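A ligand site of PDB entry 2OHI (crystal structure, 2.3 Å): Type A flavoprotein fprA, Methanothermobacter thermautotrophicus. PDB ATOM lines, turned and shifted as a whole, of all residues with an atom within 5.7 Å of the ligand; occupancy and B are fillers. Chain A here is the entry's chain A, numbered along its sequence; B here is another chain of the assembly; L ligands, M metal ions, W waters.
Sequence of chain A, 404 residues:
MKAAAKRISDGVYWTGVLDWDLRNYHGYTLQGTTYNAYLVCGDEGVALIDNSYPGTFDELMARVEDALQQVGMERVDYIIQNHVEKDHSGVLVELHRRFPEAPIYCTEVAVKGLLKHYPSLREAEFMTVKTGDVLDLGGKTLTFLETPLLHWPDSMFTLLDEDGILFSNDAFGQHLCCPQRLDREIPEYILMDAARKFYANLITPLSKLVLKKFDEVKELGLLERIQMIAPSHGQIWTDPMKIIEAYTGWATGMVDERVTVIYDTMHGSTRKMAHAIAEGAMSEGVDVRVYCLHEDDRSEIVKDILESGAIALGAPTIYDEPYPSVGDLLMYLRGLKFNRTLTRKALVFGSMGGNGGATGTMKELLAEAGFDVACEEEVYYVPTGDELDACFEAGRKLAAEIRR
O9 of the ligand lies within hydrogen-bond range of N of Met 266 (2.6 Å). O8 of the ligand sits at hydrogen-bond distance from N of Thr 270, at 2.6 Å. The side-chain hydroxyl (OG1) of Thr 270 is in hydrogen-bond range of an oxygen (O8) of the ligand. An oxygen (O8) of the ligand sits at hydrogen-bond distance from the side-chain hydroxyl (OG1) of Thr 265 (2.6 Å). The side-chain hydroxyl (OG) of Ser 351 lies within hydrogen-bond range of an oxygen (O5) of the ligand (2.7 Å). The backbone carbonyl oxygen of Thr 317 sits at hydrogen-bond distance from an oxygen (O3) of the ligand, at 2.7 Å. N of Ser 269 is in hydrogen-bond range of O7 of the ligand. N of Asp 320 is in hydrogen-bond range of O2 of the ligand (2.8 Å). An oxygen (O9) of the ligand sits at hydrogen-bond distance from the backbone NH (N) of His 267. O1 of the ligand lies within hydrogen-bond range of N of Gly 354 (2.9 Å). The backbone NH (N) of Tyr 319 sits at hydrogen-bond distance from a nitrogen (N3) of the ligand, 2.9 Å away. The backbone NH of Gly 356 sits at hydrogen-bond distance from an oxygen (O1) of the ligand. N of Gly 268 is in hydrogen-bond range of O7 of the ligand, 3.2 Å away. An oxygen (O1) of the ligand sits at hydrogen-bond distance from the backbone NH of Asn 355, at 3.3 Å. N of Gly 353 lies within hydrogen-bond range of N1 of the ligand, at 3.4 Å.
The side-chain hydroxyl (OG1) of Thr 270 sits at hydrogen-bond distance from the backbone NH (N) of Ser 351, at 3.2 Å. The side-chain hydroxyl (OG1) of Thr 265 is in hydrogen-bond range of the backbone NH (N) of Gly 268 (2.8 Å). The side-chain hydroxyl of Ser 351 sits at hydrogen-bond distance from the backbone carbonyl oxygen of Tyr 381 (2.7 Å). O of Glu 321 lies close to OG1 of Thr 317 (3.3 Å). The side-chain hydroxyl (OG) of Ser 269 sits at hydrogen-bond distance from the backbone carbonyl oxygen (O) of Tyr 381 (3.2 Å). The side-chain hydroxyl of Tyr 319 sits at hydrogen-bond distance from a ring nitrogen (ND1) of His 151 of chain B (3.2 Å). The side-chain hydroxyl of Tyr 319 is in hydrogen-bond range of the backbone carbonyl oxygen of Leu 202 of chain B, 2.6 Å away. O of Met 352 is in hydrogen-bond range of N of Tyr 381.
Pro 316 touches the ligand (CB to O6, 3.3 Å). CA of Ile 318 touches N3 of the ligand, 3.7 Å away. Met 352 touches the ligand. Tyr 381 touches the ligand. Glu 85 of chain B touches the ligand (OE1 to C9, 3.6 Å). His 151 of chain B touches the ligand. Trp 152 of chain B touches the ligand. CD2 of Leu 202 of chain B touches C7 of the ligand (3.8 Å). Hydrophobic or aromatic side chains within 4 Å of the ligand: Met 266, His 267, Pro 316, Tyr 319, Met 352, Tyr 381, His 151 of chain B, Trp 152 of chain B and Leu 202 of chain B. 22 residues have an atom within 4 Å of the ligand: Thr 265, Met 266, His 267, Gly 268, Ser 269, Thr 270, Pro 316, Thr 317, Ile 318, Tyr 319, Asp 320, Ser 351, Met 352, Gly 353, Gly 354, Asn 355, Gly 356, Tyr 381, Glu 85 of chain B, His 151 of chain B, Trp 152 of chain B and Leu 202 of chain B.
Water W2 lies within hydrogen-bond range of an oxygen (O7) of the ligand and the side-chain hydroxyl of Ser 269. Water W1 lies within hydrogen-bond range of O of Gly 356 (2.6 Å), OD1 of Asp 320 (2.6 Å) and N2 of the ligand (2.7 Å).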
ATOM      1  N   ASP A 264      -0.946   2.611  22.098  1.00  0.00           N
ATOM      2  CA  ASP A 264      -0.244   2.532  23.380  1.00  0.00           C
ATOM      3  C   ASP A 264      -0.564   3.788  24.188  1.00  0.00           C
ATOM      4  O   ASP A 264      -1.079   4.754  23.639  1.00  0.00           O
ATOM      5  CB  ASP A 264       1.263   2.336  23.213  1.00  0.00           C
ATOM      6  CG  ASP A 264       1.847   1.356  24.240  1.00  0.00           C
ATOM      7  OD1 ASP A 264       1.430   1.377  25.413  1.00  0.00           O
ATOM      8  OD2 ASP A 264       2.745   0.549  23.891  1.00  0.00           O
ATOM      9  N   THR A 265      -0.299   3.747  25.487  1.00  0.00           N
ATOM     10  CA  THR A 265      -0.582   4.866  26.370  1.00  0.00           C
ATOM     11  C   THR A 265       0.380   4.811  27.533  1.00  0.00           C
ATOM     12  O   THR A 265       0.917   3.751  27.836  1.00  0.00           O
ATOM     13  CB  THR A 265      -2.051   4.843  26.911  1.00  0.00           C
ATOM     14  OG1 THR A 265      -2.285   5.994  27.722  1.00  0.00           O
ATOM     15  CG2 THR A 265      -2.332   3.581  27.743  1.00  0.00           C
ATOM     16  N   MET A 266       0.621   5.960  28.174  1.00  0.00           N
ATOM     17  CA  MET A 266       1.381   5.990  29.441  1.00  0.00           C
ATOM     18  C   MET A 266       0.486   6.303  30.647  1.00  0.00           C
ATOM     19  O   MET A 266       0.532   5.598  31.643  1.00  0.00           O
ATOM     20  CB  MET A 266       2.541   6.962  29.362  1.00  0.00           C
ATOM     21  CG  MET A 266       3.558   6.665  28.255  1.00  0.00           C
ATOM     22  SD  MET A 266       4.832   7.942  28.204  1.00  0.00           S
ATOM     23  CE  MET A 266       3.834   9.382  27.781  1.00  0.00           C
ATOM     24  N   HIS A 267      -0.333   7.330  30.542  1.00  0.00           N
ATOM     25  CA  HIS A 267      -1.203   7.732  31.656  1.00  0.00           C
ATOM     26  C   HIS A 267      -2.683   7.452  31.382  1.00  0.00           C
ATOM     27  O   HIS A 267      -3.526   7.837  32.180  1.00  0.00           O
ATOM     28  CB  HIS A 267      -1.036   9.233  31.984  1.00  0.00           C
ATOM     29  CG  HIS A 267       0.394   9.666  32.161  1.00  0.00           C
ATOM     30  ND1 HIS A 267       1.131   9.361  33.276  1.00  0.00           N
ATOM     31  CD2 HIS A 267       1.193  10.416  31.362  1.00  0.00           C
ATOM     32  CE1 HIS A 267       2.340   9.882  33.163  1.00  0.00           C
ATOM     33  NE2 HIS A 267       2.398  10.528  32.012  1.00  0.00           N
ATOM     34  N   GLY A 268      -3.002   6.804  30.269  1.00  0.00           N
ATOM     35  CA  GLY A 268      -4.407   6.447  29.972  1.00  0.00           C
ATOM     36  C   GLY A 268      -5.250   7.376  29.109  1.00  0.00           C
ATOM     37  O   GLY A 268      -6.405   7.047  28.805  1.00  0.00           O
ATOM     38  N   SER A 269      -4.710   8.537  28.716  1.00  0.00           N
ATOM     39  CA  SER A 269      -5.482   9.495  27.892  1.00  0.00           C
ATOM     40  C   SER A 269      -5.715   9.016  26.445  1.00  0.00           C
ATOM     41  O   SER A 269      -6.824   9.129  25.957  1.00  0.00           O
ATOM     42  CB  SER A 269      -4.860  10.888  27.885  1.00  0.00           C
ATOM     43  OG  SER A 269      -5.229  11.641  29.024  1.00  0.00           O
ATOM     44  N   THR A 270      -4.683   8.498  25.772  1.00  0.00           N
ATOM     45  CA  THR A 270      -4.823   7.821  24.477  1.00  0.00           C
ATOM     46  C   THR A 270      -5.749   6.588  24.543  1.00  0.00           C
ATOM     47  O   THR A 270      -6.476   6.320  23.583  1.00  0.00           O
ATOM     48  CB  THR A 270      -3.452   7.406  23.895  1.00  0.00           C
ATOM     49  OG1 THR A 270      -2.630   8.567  23.714  1.00  0.00           O
ATOM     50  CG2 THR A 270      -3.582   6.715  22.519  1.00  0.00           C
ATOM     51  N   ARG A 271      -5.736   5.862  25.679  1.00  0.00           N
ATOM     52  CA  ARG A 271      -6.668   4.741  25.948  1.00  0.00           C
ATOM     53  C   ARG A 271      -8.144   5.178  25.949  1.00  0.00           C
ATOM     54  O   ARG A 271      -8.994   4.528  25.338  1.00  0.00           O
ATOM     55  CB  ARG A 271      -6.310   4.042  27.274  1.00  0.00           C
ATOM     56  CG  ARG A 271      -7.437   3.167  27.896  1.00  0.00           C
ATOM     57  CD  ARG A 271      -6.934   2.033  28.808  1.00  0.00           C
ATOM     58  NE  ARG A 271      -5.993   2.465  29.848  1.00  0.00           N
ATOM     59  CZ  ARG A 271      -4.776   1.944  30.045  1.00  0.00           C
ATOM     60  NH1 ARG A 271      -4.318   0.946  29.289  1.00  0.00           N
ATOM     61  NH2 ARG A 271      -4.003   2.406  31.020  1.00  0.00           N
ATOM     62  N   PRO A 316       0.644   8.317  22.576  1.00  0.00           N
ATOM     63  CA  PRO A 316       1.049   9.626  23.069  1.00  0.00           C
ATOM     64  C   PRO A 316       2.412   9.999  22.487  1.00  0.00           C
ATOM     65  O   PRO A 316       3.124   9.123  22.039  1.00  0.00           O
ATOM     66  CB  PRO A 316       1.129   9.414  24.571  1.00  0.00           C
ATOM     67  CG  PRO A 316       1.520   7.985  24.705  1.00  0.00           C
ATOM     68  CD  PRO A 316       0.786   7.271  23.611  1.00  0.00           C
ATOM     69  N   THR A 317       2.754  11.275  22.486  1.00  0.00           N
ATOM     70  CA  THR A 317       4.045  11.744  22.029  1.00  0.00           C
ATOM     71  C   THR A 317       5.036  11.873  23.197  1.00  0.00           C
ATOM     72  O   THR A 317       4.682  12.285  24.309  1.00  0.00           O
ATOM     73  CB  THR A 317       3.940  13.024  21.169  1.00  0.00           C
ATOM     74  OG1 THR A 317       5.224  13.642  21.055  1.00  0.00           O
ATOM     75  CG2 THR A 317       3.019  13.989  21.766  1.00  0.00           C
ATOM     76  N   ILE A 318       6.262  11.466  22.905  1.00  0.00           N
ATOM     77  CA  ILE A 318       7.308  11.326  23.884  1.00  0.00           C
ATOM     78  C   ILE A 318       8.542  11.860  23.214  1.00  0.00           C
ATOM     79  O   ILE A 318       9.050  11.276  22.265  1.00  0.00           O
ATOM     80  CB  ILE A 318       7.498   9.820  24.288  1.00  0.00           C
ATOM     81  CG1 ILE A 318       6.326   9.333  25.126  1.00  0.00           C
ATOM     82  CG2 ILE A 318       8.810   9.566  25.085  1.00  0.00           C
ATOM     83  CD1 ILE A 318       6.552   7.953  25.708  1.00  0.00           C
ATOM     84  N   TYR A 319       9.001  13.002  23.685  1.00  0.00           N
ATOM     85  CA  TYR A 319      10.181  13.662  23.124  1.00  0.00           C
ATOM     86  C   TYR A 319      10.122  13.853  21.599  1.00  0.00           C
ATOM     87  O   TYR A 319      11.115  13.645  20.907  1.00  0.00           O
ATOM     88  CB  TYR A 319      11.475  12.986  23.621  1.00  0.00           C
ATOM     89  CG  TYR A 319      11.697  13.195  25.105  1.00  0.00           C
ATOM     90  CD1 TYR A 319      11.449  14.447  25.677  1.00  0.00           C
ATOM     91  CD2 TYR A 319      12.132  12.163  25.940  1.00  0.00           C
ATOM     92  CE1 TYR A 319      11.636  14.674  27.029  1.00  0.00           C
ATOM     93  CE2 TYR A 319      12.322  12.384  27.313  1.00  0.00           C
ATOM     94  CZ  TYR A 319      12.078  13.649  27.846  1.00  0.00           C
ATOM     95  OH  TYR A 319      12.232  13.936  29.198  1.00  0.00           O
ATOM     96  N   ASP A 320       8.960  14.282  21.100  1.00  0.00           N
ATOM     97  CA  ASP A 320       8.741  14.574  19.679  1.00  0.00           C
ATOM     98  C   ASP A 320       8.517  13.337  18.804  1.00  0.00           C
ATOM     99  O   ASP A 320       8.524  13.436  17.577  1.00  0.00           O
ATOM    100  CB  ASP A 320       9.900  15.402  19.084  1.00  0.00           C
ATOM    101  CG  ASP A 320       9.790  16.885  19.378  1.00  0.00           C
ATOM    102  OD1 ASP A 320       8.761  17.356  19.909  1.00  0.00           O
ATOM    103  OD2 ASP A 320      10.757  17.613  19.058  1.00  0.00           O
ATOM    104  N   GLU A 321       8.335  12.190  19.434  1.00  0.00           N
ATOM    105  CA  GLU A 321       8.160  10.920  18.737  1.00  0.00           C
ATOM    106  C   GLU A 321       6.906  10.240  19.296  1.00  0.00           C
ATOM    107  O   GLU A 321       6.441  10.600  20.390  1.00  0.00           O
ATOM    108  CB  GLU A 321       9.368  10.002  18.968  1.00  0.00           C
ATOM    109  CG  GLU A 321      10.708  10.535  18.441  1.00  0.00           C
ATOM    110  CD  GLU A 321      10.794  10.644  16.905  1.00  0.00           C
ATOM    111  OE1 GLU A 321      10.101   9.888  16.199  1.00  0.00           O
ATOM    112  OE2 GLU A 321      11.576  11.486  16.422  1.00  0.00           O
ATOM    113  N   SER A 351      -2.971  11.489  22.533  1.00  0.00           N
ATOM    114  CA  SER A 351      -2.870  12.609  23.451  1.00  0.00           C
ATOM    115  C   SER A 351      -1.448  13.125  23.509  1.00  0.00           C
ATOM    116  O   SER A 351      -0.507  12.410  23.157  1.00  0.00           O
ATOM    117  CB  SER A 351      -3.357  12.205  24.840  1.00  0.00           C
ATOM    118  OG  SER A 351      -3.063  13.172  25.817  1.00  0.00           O
ATOM    119  N   MET A 352      -1.292  14.370  23.926  1.00  0.00           N
ATOM    120  CA  MET A 352       0.011  14.998  24.040  1.00  0.00           C
ATOM    121  C   MET A 352      -0.080  16.150  25.034  1.00  0.00           C
ATOM    122  O   MET A 352      -1.175  16.498  25.490  1.00  0.00           O
ATOM    123  CB  MET A 352       0.533  15.444  22.670  1.00  0.00           C
ATOM    124  CG  MET A 352      -0.442  16.244  21.820  1.00  0.00           C
ATOM    125  SD  MET A 352      -0.298  18.027  22.091  1.00  0.00           S
ATOM    126  CE  MET A 352      -1.965  18.570  21.670  1.00  0.00           C
ATOM    127  N   GLY A 353       1.068  16.732  25.378  1.00  0.00           N
ATOM    128  CA  GLY A 353       1.110  17.818  26.339  1.00  0.00           C
ATOM    129  C   GLY A 353       1.895  19.068  25.973  1.00  0.00           C
ATOM    130  O   GLY A 353       2.112  19.930  26.822  1.00  0.00           O
ATOM    131  N   GLY A 354       2.321  19.183  24.720  1.00  0.00           N
ATOM    132  CA  GLY A 354       3.143  20.312  24.320  1.00  0.00           C
ATOM    133  C   GLY A 354       2.981  20.657  22.862  1.00  0.00           C
ATOM    134  O   GLY A 354       2.003  21.314  22.491  1.00  0.00           O
ATOM    135  N   ASN A 355       3.942  20.234  22.038  1.00  0.00           N
ATOM    136  CA  ASN A 355       3.926  20.477  20.596  1.00  0.00           C
ATOM    137  C   ASN A 355       3.332  19.315  19.813  1.00  0.00           C
ATOM    138  O   ASN A 355       2.958  19.464  18.652  1.00  0.00           O
ATOM    139  CB  ASN A 355       5.349  20.707  20.084  1.00  0.00           C
ATOM    140  CG  ASN A 355       5.809  22.127  20.242  1.00  0.00           C
ATOM    141  OD1 ASN A 355       7.013  22.417  20.150  1.00  0.00           O
ATOM    142  ND2 ASN A 355       4.864  23.035  20.464  1.00  0.00           N
ATOM    143  N   GLY A 356       3.249  18.154  20.464  1.00  0.00           N
ATOM    144  CA  GLY A 356       2.777  16.943  19.812  1.00  0.00           C
ATOM    145  C   GLY A 356       3.819  16.411  18.840  1.00  0.00           C
ATOM    146  O   GLY A 356       5.012  16.544  19.081  1.00  0.00           O
ATOM    147  N   GLY A 357       3.353  15.801  17.742  1.00  0.00           N
ATOM    148  CA  GLY A 357       4.258  15.281  16.710  1.00  0.00           C
ATOM    149  C   GLY A 357       4.156  13.793  16.434  1.00  0.00           C
ATOM    150  O   GLY A 357       4.573  13.323  15.358  1.00  0.00           O
ATOM    151  N   TYR A 380      -5.024  17.604  23.714  1.00  0.00           N
ATOM    152  CA  TYR A 380      -4.138  18.101  24.758  1.00  0.00           C
ATOM    153  C   TYR A 380      -4.470  17.420  26.086  1.00  0.00           C
ATOM    154  O   TYR A 380      -5.576  17.554  26.602  1.00  0.00           O
ATOM    155  CB  TYR A 380      -4.273  19.611  24.869  1.00  0.00           C
ATOM    156  CG  TYR A 380      -3.360  20.278  25.865  1.00  0.00           C
ATOM    157  CD1 TYR A 380      -3.892  21.085  26.871  1.00  0.00           C
ATOM    158  CD2 TYR A 380      -1.968  20.106  25.800  1.00  0.00           C
ATOM    159  CE1 TYR A 380      -3.066  21.723  27.788  1.00  0.00           C
ATOM    160  CE2 TYR A 380      -1.132  20.735  26.717  1.00  0.00           C
ATOM    161  CZ  TYR A 380      -1.691  21.542  27.712  1.00  0.00           C
ATOM    162  OH  TYR A 380      -0.878  22.177  28.634  1.00  0.00           O
ATOM    163  N   TYR A 381      -3.502  16.673  26.623  1.00  0.00           N
ATOM    164  CA  TYR A 381      -3.611  15.953  27.908  1.00  0.00           C
ATOM    165  C   TYR A 381      -4.886  15.108  28.004  1.00  0.00           C
ATOM    166  O   TYR A 381      -5.094  14.246  27.159  1.00  0.00           O
ATOM    167  CB  TYR A 381      -3.436  16.903  29.107  1.00  0.00           C
ATOM    168  CG  TYR A 381      -1.998  17.372  29.371  1.00  0.00           C
ATOM    169  CD1 TYR A 381      -0.919  16.497  29.328  1.00  0.00           C
ATOM    170  CD2 TYR A 381      -1.743  18.704  29.700  1.00  0.00           C
ATOM    171  CE1 TYR A 381       0.376  16.919  29.575  1.00  0.00           C
ATOM    172  CE2 TYR A 381      -0.447  19.149  29.945  1.00  0.00           C
ATOM    173  CZ  TYR A 381       0.615  18.255  29.888  1.00  0.00           C
ATOM    174  OH  TYR A 381       1.904  18.692  30.150  1.00  0.00           O
ATOM    175  N   VAL A 382      -5.707  15.336  29.022  1.00  0.00           N
ATOM    176  CA  VAL A 382      -6.910  14.514  29.236  1.00  0.00           C
ATOM    177  C   VAL A 382      -8.051  15.014  28.351  1.00  0.00           C
ATOM    178  O   VAL A 382      -8.348  16.203  28.364  1.00  0.00           O
ATOM    179  CB  VAL A 382      -7.349  14.494  30.739  1.00  0.00           C
ATOM    180  CG1 VAL A 382      -8.613  13.666  30.915  1.00  0.00           C
ATOM    181  CG2 VAL A 382      -6.216  13.911  31.645  1.00  0.00           C
ATOM    182  N   HIS B  26       5.516   3.365  32.636  1.00  0.00           N
ATOM    183  CA  HIS B  26       5.425   3.762  31.214  1.00  0.00           C
ATOM    184  C   HIS B  26       6.625   3.383  30.329  1.00  0.00           C
ATOM    185  O   HIS B  26       7.253   4.245  29.690  1.00  0.00           O
ATOM    186  CB  HIS B  26       4.969   5.234  31.049  1.00  0.00           C
ATOM    187  CG  HIS B  26       5.920   6.275  31.556  1.00  0.00           C
ATOM    188  ND1 HIS B  26       5.560   7.202  32.504  1.00  0.00           N
ATOM    189  CD2 HIS B  26       7.206   6.551  31.227  1.00  0.00           C
ATOM    190  CE1 HIS B  26       6.596   8.005  32.744  1.00  0.00           C
ATOM    191  NE2 HIS B  26       7.604   7.628  31.991  1.00  0.00           N
ATOM    192  N   GLU B  85       2.537  16.545  35.880  1.00  0.00           N
ATOM    193  CA  GLU B  85       2.417  15.112  35.620  1.00  0.00           C
ATOM    194  C   GLU B  85       1.623  14.396  36.732  1.00  0.00           C
ATOM    195  O   GLU B  85       1.728  14.747  37.907  1.00  0.00           O
ATOM    196  CB  GLU B  85       3.785  14.473  35.383  1.00  0.00           C
ATOM    197  CG  GLU B  85       3.727  13.074  34.772  1.00  0.00           C
ATOM    198  CD  GLU B  85       5.088  12.535  34.331  1.00  0.00           C
ATOM    199  OE1 GLU B  85       5.776  13.256  33.570  1.00  0.00           O
ATOM    200  OE2 GLU B  85       5.469  11.409  34.731  1.00  0.00           O
ATOM    201  N   HIS B 151      11.535  18.660  33.315  1.00  0.00           N
ATOM    202  CA  HIS B 151      11.489  17.963  32.026  1.00  0.00           C
ATOM    203  C   HIS B 151      10.264  18.236  31.144  1.00  0.00           C
ATOM    204  O   HIS B 151      10.155  17.690  30.039  1.00  0.00           O
ATOM    205  CB  HIS B 151      11.765  16.457  32.211  1.00  0.00           C
ATOM    206  CG  HIS B 151      10.538  15.615  32.350  1.00  0.00           C
ATOM    207  ND1 HIS B 151      10.081  14.794  31.344  1.00  0.00           N
ATOM    208  CD2 HIS B 151       9.687  15.433  33.400  1.00  0.00           C
ATOM    209  CE1 HIS B 151       9.003  14.146  31.756  1.00  0.00           C
ATOM    210  NE2 HIS B 151       8.746  14.516  33.003  1.00  0.00           N
ATOM    211  N   TRP B 152       9.356  19.103  31.627  1.00  0.00           N
ATOM    212  CA  TRP B 152       8.151  19.524  30.881  1.00  0.00           C
ATOM    213  C   TRP B 152       8.018  21.058  30.797  1.00  0.00           C
ATOM    214  O   TRP B 152       8.532  21.777  31.658  1.00  0.00           O
ATOM    215  CB  TRP B 152       6.890  18.927  31.538  1.00  0.00           C
ATOM    216  CG  TRP B 152       6.520  17.503  31.150  1.00  0.00           C
ATOM    217  CD1 TRP B 152       7.309  16.577  30.506  1.00  0.00           C
ATOM    218  CD2 TRP B 152       5.282  16.827  31.420  1.00  0.00           C
ATOM    219  NE1 TRP B 152       6.627  15.400  30.358  1.00  0.00           N
ATOM    220  CE2 TRP B 152       5.389  15.524  30.910  1.00  0.00           C
ATOM    221  CE3 TRP B 152       4.077  17.219  32.045  1.00  0.00           C
ATOM    222  CZ2 TRP B 152       4.333  14.585  30.997  1.00  0.00           C
ATOM    223  CZ3 TRP B 152       3.043  16.284  32.131  1.00  0.00           C
ATOM    224  CH2 TRP B 152       3.175  14.988  31.611  1.00  0.00           C
ATOM    225  N   ASN B 201      17.117   7.906  30.407  1.00  0.00           N
ATOM    226  CA  ASN B 201      15.772   7.778  29.869  1.00  0.00           C
ATOM    227  C   ASN B 201      14.991   9.098  29.826  1.00  0.00           C
ATOM    228  O   ASN B 201      14.052   9.212  29.095  1.00  0.00           O
ATOM    229  CB  ASN B 201      14.980   6.691  30.629  1.00  0.00           C
ATOM    230  CG  ASN B 201      15.517   5.301  30.366  1.00  0.00           C
ATOM    231  OD1 ASN B 201      15.045   4.639  29.451  1.00  0.00           O
ATOM    232  ND2 ASN B 201      16.530   4.865  31.135  1.00  0.00           N
ATOM    233  N   LEU B 202      15.399  10.090  30.594  1.00  0.00           N
ATOM    234  CA  LEU B 202      14.532  11.247  30.774  1.00  0.00           C
ATOM    235  C   LEU B 202      15.227  12.594  30.525  1.00  0.00           C
ATOM    236  O   LEU B 202      14.621  13.531  30.021  1.00  0.00           O
ATOM    237  CB  LEU B 202      13.875  11.187  32.176  1.00  0.00           C
ATOM    238  CG  LEU B 202      12.820  10.071  32.376  1.00  0.00           C
ATOM    239  CD1 LEU B 202      12.341   9.957  33.792  1.00  0.00           C
ATOM    240  CD2 LEU B 202      11.601  10.263  31.453  1.00  0.00           C
HETATM  241  N1  LIG L   1       4.279  15.783  24.887  1.00  0.00           N
HETATM  242  C1  LIG L   1       4.580  16.549  23.798  1.00  0.00           C
HETATM  243  O1  LIG L   1       3.699  17.157  23.206  1.00  0.00           O
HETATM  244  N2  LIG L   1       5.884  16.626  23.374  1.00  0.00           N
HETATM  245  C2  LIG L   1       6.903  15.963  23.998  1.00  0.00           C
HETATM  246  O2  LIG L   1       7.875  15.761  23.278  1.00  0.00           O
HETATM  247  C3  LIG L   1       6.607  15.171  25.102  1.00  0.00           C
HETATM  248  N3  LIG L   1       7.571  14.460  25.812  1.00  0.00           N
HETATM  249  C4  LIG L   1       7.204  13.684  26.906  1.00  0.00           C
HETATM  250  C5  LIG L   1       8.150  12.953  27.635  1.00  0.00           C
HETATM  251  C6  LIG L   1       7.800  12.163  28.741  1.00  0.00           C
HETATM  252  C7  LIG L   1       8.700  11.018  29.106  1.00  0.00           C
HETATM  253  C8  LIG L   1       6.473  12.103  29.140  1.00  0.00           C
HETATM  254  C9  LIG L   1       6.081  11.447  30.432  1.00  0.00           C
HETATM  255  C10 LIG L   1       5.511  12.827  28.425  1.00  0.00           C
HETATM  256  C11 LIG L   1       5.875  13.610  27.310  1.00  0.00           C
HETATM  257  N4  LIG L   1       4.908  14.317  26.609  1.00  0.00           N
HETATM  258  C12 LIG L   1       5.276  15.097  25.540  1.00  0.00           C
HETATM  259  C13 LIG L   1       3.522  14.477  27.152  1.00  0.00           C
HETATM  260  C14 LIG L   1       2.559  13.382  26.733  1.00  0.00           C
HETATM  261  O3  LIG L   1       2.412  13.360  25.329  1.00  0.00           O
HETATM  262  C15 LIG L   1       1.231  13.669  27.429  1.00  0.00           C
HETATM  263  O4  LIG L   1       1.436  13.693  28.822  1.00  0.00           O
HETATM  264  C16 LIG L   1       0.059  12.746  27.043  1.00  0.00           C
HETATM  265  O5  LIG L   1      -1.127  13.214  27.672  1.00  0.00           O
HETATM  266  C17 LIG L   1       0.233  11.260  27.379  1.00  0.00           C
HETATM  267  O6  LIG L   1      -0.887  10.563  26.886  1.00  0.00           O
HETATM  268  P1  LIG L   1      -1.348   9.195  27.548  1.00  0.00           P
HETATM  269  O7  LIG L   1      -2.181   9.547  28.760  1.00  0.00           O
HETATM  270  O8  LIG L   1      -2.204   8.382  26.631  1.00  0.00           O
HETATM  271  O9  LIG L   1      -0.119   8.426  27.915  1.00  0.00           O
HETATM  272 FE    FE M   1       7.505  14.113  34.946  1.00  0.00          FE
HETATM  273  O   HOH W   1       6.396  17.739  20.915  1.00  0.00           O
HETATM  274  O   HOH W   2      -2.415  11.970  29.812  1.00  0.00           O
